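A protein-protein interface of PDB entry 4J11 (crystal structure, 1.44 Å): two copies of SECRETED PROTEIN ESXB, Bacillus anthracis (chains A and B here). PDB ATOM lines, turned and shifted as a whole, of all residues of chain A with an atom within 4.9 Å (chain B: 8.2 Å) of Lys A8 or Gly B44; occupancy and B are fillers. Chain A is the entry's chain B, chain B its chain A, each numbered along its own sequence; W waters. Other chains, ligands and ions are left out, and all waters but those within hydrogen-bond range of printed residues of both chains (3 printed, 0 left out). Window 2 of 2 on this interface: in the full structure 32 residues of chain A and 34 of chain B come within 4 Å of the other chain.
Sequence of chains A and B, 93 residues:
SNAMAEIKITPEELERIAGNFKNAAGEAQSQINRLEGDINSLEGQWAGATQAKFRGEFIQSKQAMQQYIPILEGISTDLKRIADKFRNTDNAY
O of Gln B45 is in hydrogen-bond range of N of Lys A8 (2.8 Å). O of Glu A6 sits close to O of Gln B45, 3.4 Å away.
The backbone carbonyl oxygen (O) of Leu B42 sits close to the indole nitrogen (NE1) of Trp B46, 3.5 Å away. The side-chain amide oxygen (OE1) of Gln B51 lies within hydrogen-bond range of the indole nitrogen (NE1) of Trp B46 (2.8 Å).
O of Glu A6 touches CA of Trp B46 (3.4 Å). Glu A6 touches Ala B47 (OE1 to CA, 3.7 Å). O of Gln B45 touches CA of Ile A7, at 3.7 Å. Gly B44 touches Lys A8 (O to CD, 3.6 Å). Ile A9 touches Leu B42. Ile A9 touches Gln B45 (N to O, 3.8 Å).
Printed residues of chain B within 4 Å of Glu A6: Gln B45, Trp B46 and Ala B47. Of chain B, only Gly B44 (3.6 Å) and Gln B45 (2.8 Å) come within 4 Å of Lys A8. Of the printed residues of chain B, Ile A9 touches Leu B42 and Gln B45. Of chain A, only Lys A8 (3.6 Å) comes within 4 Å of Gly B44. Of the printed residues of chain A, Gln B45 touches Glu A6, Ile A7, Lys A8 and Ile A9. Printed residues of chain A within 4 Å of Trp B46: Glu A6 (3.4 Å). Of the printed residues of chain A, Ala B47 touches Glu A6 (3.7 Å). Gly B48 touches none of the printed residues of chain A. Gln B51 touches none of the printed residues of chain A. The nearest printed residue of chain B that does not touch Glu A6 is Gly B44 (4.6 Å).
Printed residues of chain B that touch a printed residue of chain A: Leu B42, Gly B44, Gln B45, Trp B46 and Ala B47. Hydrophobic or aromatic side chains of chain B within 4 Å of the printed part of chain A: Leu B42 and Ala B47. Among the printed residues, 8 pairs touch across the chains.
No position is printed for both chains. Of the 8 pairs that touch across the chains among the printed residues, none has its exchanged pair printed and touching as well.
Water W1 bridges the backbone carbonyl oxygen of Glu A6 and the backbone carbonyl oxygen of Gly B44. Water W2 lies within hydrogen-bond range of the backbone carbonyl oxygen of Gly B44 (2.7 Å) and the side-chain amino group of Lys A8 (2.9 Å). Water W3 bridges N of Gly B48 and OE1 of Glu A6.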
ATOM      1  N   ALA A   5       1.376  27.782 -15.921  1.00  0.00           N
ATOM      2  CA  ALA A   5       0.757  29.090 -16.142  1.00  0.00           C
ATOM      3  C   ALA A   5      -0.416  29.062 -17.118  1.00  0.00           C
ATOM      4  O   ALA A   5      -1.369  29.832 -16.969  1.00  0.00           O
ATOM      5  CB  ALA A   5       1.793  30.103 -16.594  1.00  0.00           C
ATOM      6  N   GLU A   6      -0.341  28.181 -18.109  1.00  0.00           N
ATOM      7  CA  GLU A   6      -1.405  28.038 -19.103  1.00  0.00           C
ATOM      8  C   GLU A   6      -2.743  27.601 -18.497  1.00  0.00           C
ATOM      9  O   GLU A   6      -3.823  27.900 -19.035  1.00  0.00           O
ATOM     10  CB  GLU A   6      -0.975  27.049 -20.195  1.00  0.00           C
ATOM     11  CG  GLU A   6      -2.011  26.831 -21.287  1.00  0.00           C
ATOM     12  CD  GLU A   6      -1.511  25.946 -22.409  1.00  0.00           C
ATOM     13  OE1 GLU A   6      -1.479  26.419 -23.565  1.00  0.00           O
ATOM     14  OE2 GLU A   6      -1.161  24.778 -22.141  1.00  0.00           O
ATOM     15  N   ILE A   7      -2.679  26.904 -17.364  1.00  0.00           N
ATOM     16  CA  ILE A   7      -3.879  26.412 -16.704  1.00  0.00           C
ATOM     17  C   ILE A   7      -4.272  27.398 -15.615  1.00  0.00           C
ATOM     18  O   ILE A   7      -3.634  27.460 -14.545  1.00  0.00           O
ATOM     19  CB  ILE A   7      -3.662  24.997 -16.117  1.00  0.00           C
ATOM     20  CG1 ILE A   7      -3.340  23.992 -17.227  1.00  0.00           C
ATOM     21  CG2 ILE A   7      -4.887  24.544 -15.344  1.00  0.00           C
ATOM     22  CD1 ILE A   7      -2.903  22.631 -16.703  1.00  0.00           C
ATOM     23  N   LYS A   8      -5.307  28.186 -15.889  1.00  0.00           N
ATOM     24  CA  LYS A   8      -5.702  29.268 -14.987  1.00  0.00           C
ATOM     25  C   LYS A   8      -6.981  28.952 -14.235  1.00  0.00           C
ATOM     26  O   LYS A   8      -7.564  29.828 -13.597  1.00  0.00           O
ATOM     27  CB  LYS A   8      -5.841  30.577 -15.764  1.00  0.00           C
ATOM     28  CG  LYS A   8      -4.578  30.930 -16.547  1.00  0.00           C
ATOM     29  CD  LYS A   8      -4.673  32.277 -17.245  1.00  0.00           C
ATOM     30  CE  LYS A   8      -3.366  32.614 -17.947  1.00  0.00           C
ATOM     31  NZ  LYS A   8      -3.334  34.024 -18.424  1.00  0.00           N
ATOM     32  N   ILE A   9      -7.394  27.692 -14.298  1.00  0.00           N
ATOM     33  CA  ILE A   9      -8.609  27.240 -13.634  1.00  0.00           C
ATOM     34  C   ILE A   9      -8.312  26.033 -12.741  1.00  0.00           C
ATOM     35  O   ILE A   9      -7.483  25.183 -13.082  1.00  0.00           O
ATOM     36  CB  ILE A   9      -9.720  26.933 -14.683  1.00  0.00           C
ATOM     37  CG1 ILE A   9     -11.048  26.648 -13.997  1.00  0.00           C
ATOM     38  CG2 ILE A   9      -9.305  25.788 -15.635  1.00  0.00           C
ATOM     39  CD1 ILE A   9     -12.246  26.749 -14.903  1.00  0.00           C
ATOM     40  N   THR A  10      -8.974  25.976 -11.590  1.00  0.00           N
ATOM     41  CA  THR A  10      -8.777  24.876 -10.652  1.00  0.00           C
ATOM     42  C   THR A  10      -9.714  23.704 -10.979  1.00  0.00           C
ATOM     43  O   THR A  10     -10.739  23.874 -11.669  1.00  0.00           O
ATOM     44  CB  THR A  10      -9.097  25.315  -9.221  1.00  0.00           C
ATOM     45  OG1 THR A  10     -10.452  25.752  -9.183  1.00  0.00           O
ATOM     46  CG2 THR A  10      -8.173  26.438  -8.746  1.00  0.00           C
ATOM     47  N   ILE B  39     -18.931  28.710 -21.184  1.00  0.00           N
ATOM     48  CA  ILE B  39     -17.946  28.421 -22.215  1.00  0.00           C
ATOM     49  C   ILE B  39     -17.073  29.655 -22.492  1.00  0.00           C
ATOM     50  O   ILE B  39     -15.855  29.551 -22.633  1.00  0.00           O
ATOM     51  CB  ILE B  39     -18.650  27.934 -23.500  1.00  0.00           C
ATOM     52  CG1 ILE B  39     -19.427  26.639 -23.231  1.00  0.00           C
ATOM     53  CG2 ILE B  39     -17.646  27.715 -24.605  1.00  0.00           C
ATOM     54  CD1 ILE B  39     -18.563  25.453 -22.808  1.00  0.00           C
ATOM     55  N   ASN B  40     -17.699  30.832 -22.559  1.00  0.00           N
ATOM     56  CA  ASN B  40     -16.944  32.073 -22.752  1.00  0.00           C
ATOM     57  C   ASN B  40     -15.922  32.293 -21.641  1.00  0.00           C
ATOM     58  O   ASN B  40     -14.826  32.806 -21.888  1.00  0.00           O
ATOM     59  CB  ASN B  40     -17.874  33.294 -22.815  1.00  0.00           C
ATOM     60  CG  ASN B  40     -18.676  33.357 -24.094  1.00  0.00           C
ATOM     61  OD1 ASN B  40     -18.341  32.706 -25.081  1.00  0.00           O
ATOM     62  ND2 ASN B  40     -19.742  34.157 -24.087  1.00  0.00           N
ATOM     63  N   SER B  41     -16.285  31.904 -20.419  1.00  0.00           N
ATOM     64  CA  SER B  41     -15.425  32.131 -19.256  1.00  0.00           C
ATOM     65  C   SER B  41     -14.156  31.289 -19.283  1.00  0.00           C
ATOM     66  O   SER B  41     -13.176  31.626 -18.623  1.00  0.00           O
ATOM     67  CB  SER B  41     -16.193  31.908 -17.940  1.00  0.00           C
ATOM     68  OG  SER B  41     -16.390  30.527 -17.643  1.00  0.00           O
ATOM     69  N   LEU B  42     -14.182  30.201 -20.049  1.00  0.00           N
ATOM     70  CA  LEU B  42     -13.053  29.281 -20.137  1.00  0.00           C
ATOM     71  C   LEU B  42     -12.006  29.714 -21.152  1.00  0.00           C
ATOM     72  O   LEU B  42     -10.868  29.251 -21.120  1.00  0.00           O
ATOM     73  CB  LEU B  42     -13.537  27.869 -20.452  1.00  0.00           C
ATOM     74  CG  LEU B  42     -14.283  27.195 -19.300  1.00  0.00           C
ATOM     75  CD1 LEU B  42     -15.067  25.984 -19.759  1.00  0.00           C
ATOM     76  CD2 LEU B  42     -13.304  26.790 -18.224  1.00  0.00           C
ATOM     77  N   GLU B  43     -12.386  30.624 -22.041  1.00  0.00           N
ATOM     78  CA  GLU B  43     -11.452  31.122 -23.045  1.00  0.00           C
ATOM     79  C   GLU B  43     -10.232  31.722 -22.367  1.00  0.00           C
ATOM     80  O   GLU B  43     -10.357  32.567 -21.481  1.00  0.00           O
ATOM     81  CB  GLU B  43     -12.127  32.161 -23.942  1.00  0.00           C
ATOM     82  CG  GLU B  43     -11.168  32.919 -24.851  1.00  0.00           C
ATOM     83  CD  GLU B  43     -10.496  32.039 -25.896  1.00  0.00           C
ATOM     84  OE1 GLU B  43      -9.463  32.463 -26.459  1.00  0.00           O
ATOM     85  OE2 GLU B  43     -11.003  30.933 -26.170  1.00  0.00           O
ATOM     86  N   GLY B  44      -9.054  31.252 -22.761  1.00  0.00           N
ATOM     87  CA  GLY B  44      -7.807  31.758 -22.223  1.00  0.00           C
ATOM     88  C   GLY B  44      -7.410  31.133 -20.899  1.00  0.00           C
ATOM     89  O   GLY B  44      -6.344  31.447 -20.365  1.00  0.00           O
ATOM     90  N   GLN B  45      -8.247  30.245 -20.367  1.00  0.00           N
ATOM     91  CA  GLN B  45      -8.000  29.660 -19.046  1.00  0.00           C
ATOM     92  C   GLN B  45      -7.337  28.288 -19.106  1.00  0.00           C
ATOM     93  O   GLN B  45      -7.039  27.689 -18.068  1.00  0.00           O
ATOM     94  CB  GLN B  45      -9.311  29.523 -18.265  1.00  0.00           C
ATOM     95  CG  GLN B  45     -10.025  30.821 -17.957  1.00  0.00           C
ATOM     96  CD  GLN B  45      -9.461  31.505 -16.739  1.00  0.00           C
ATOM     97  OE1 GLN B  45      -9.802  31.165 -15.603  1.00  0.00           O
ATOM     98  NE2 GLN B  45      -8.582  32.473 -16.965  1.00  0.00           N
ATOM     99  N   TRP B  46      -7.150  27.785 -20.323  1.00  0.00           N
ATOM    100  CA  TRP B  46      -6.543  26.477 -20.563  1.00  0.00           C
ATOM    101  C   TRP B  46      -6.088  26.415 -22.026  1.00  0.00           C
ATOM    102  O   TRP B  46      -6.247  27.397 -22.751  1.00  0.00           O
ATOM    103  CB  TRP B  46      -7.508  25.334 -20.187  1.00  0.00           C
ATOM    104  CG  TRP B  46      -8.876  25.369 -20.865  1.00  0.00           C
ATOM    105  CD1 TRP B  46      -9.304  26.248 -21.831  1.00  0.00           C
ATOM    106  CD2 TRP B  46      -9.987  24.498 -20.598  1.00  0.00           C
ATOM    107  NE1 TRP B  46     -10.604  25.966 -22.184  1.00  0.00           N
ATOM    108  CE2 TRP B  46     -11.036  24.891 -21.459  1.00  0.00           C
ATOM    109  CE3 TRP B  46     -10.185  23.410 -19.739  1.00  0.00           C
ATOM    110  CZ2 TRP B  46     -12.284  24.251 -21.452  1.00  0.00           C
ATOM    111  CZ3 TRP B  46     -11.420  22.767 -19.751  1.00  0.00           C
ATOM    112  CH2 TRP B  46     -12.451  23.194 -20.598  1.00  0.00           C
ATOM    113  N   ALA B  47      -5.514  25.286 -22.452  1.00  0.00           N
ATOM    114  CA  ALA B  47      -4.968  25.148 -23.812  1.00  0.00           C
ATOM    115  C   ALA B  47      -6.003  25.475 -24.884  1.00  0.00           C
ATOM    116  O   ALA B  47      -7.167  25.117 -24.764  1.00  0.00           O
ATOM    117  CB  ALA B  47      -4.434  23.749 -24.024  1.00  0.00           C
ATOM    118  N   GLY B  48      -5.565  26.155 -25.937  1.00  0.00           N
ATOM    119  CA  GLY B  48      -6.437  26.487 -27.049  1.00  0.00           C
ATOM    120  C   GLY B  48      -7.119  25.285 -27.681  1.00  0.00           C
ATOM    121  O   GLY B  48      -8.272  25.367 -28.100  1.00  0.00           O
ATOM    122  N   GLN B  51     -10.094  24.460 -25.429  1.00  0.00           N
ATOM    123  CA  GLN B  51     -11.174  25.412 -25.672  1.00  0.00           C
ATOM    124  C   GLN B  51     -11.897  25.168 -26.996  1.00  0.00           C
ATOM    125  O   GLN B  51     -13.116  25.274 -27.061  1.00  0.00           O
ATOM    126  CB  GLN B  51     -10.650  26.850 -25.626  1.00  0.00           C
ATOM    127  CG  GLN B  51     -11.723  27.910 -25.804  1.00  0.00           C
ATOM    128  CD  GLN B  51     -12.733  27.950 -24.673  1.00  0.00           C
ATOM    129  OE1 GLN B  51     -12.539  27.331 -23.620  1.00  0.00           O
ATOM    130  NE2 GLN B  51     -13.807  28.696 -24.877  1.00  0.00           N
HETATM  131  O   HOH W   1      -4.020  29.960 -20.611  1.00  0.00           O
HETATM  132  O   HOH W   2      -5.320  33.963 -20.488  1.00  0.00           O
HETATM  133  O   HOH W   3      -2.941  27.167 -26.072  1.00  0.00           O
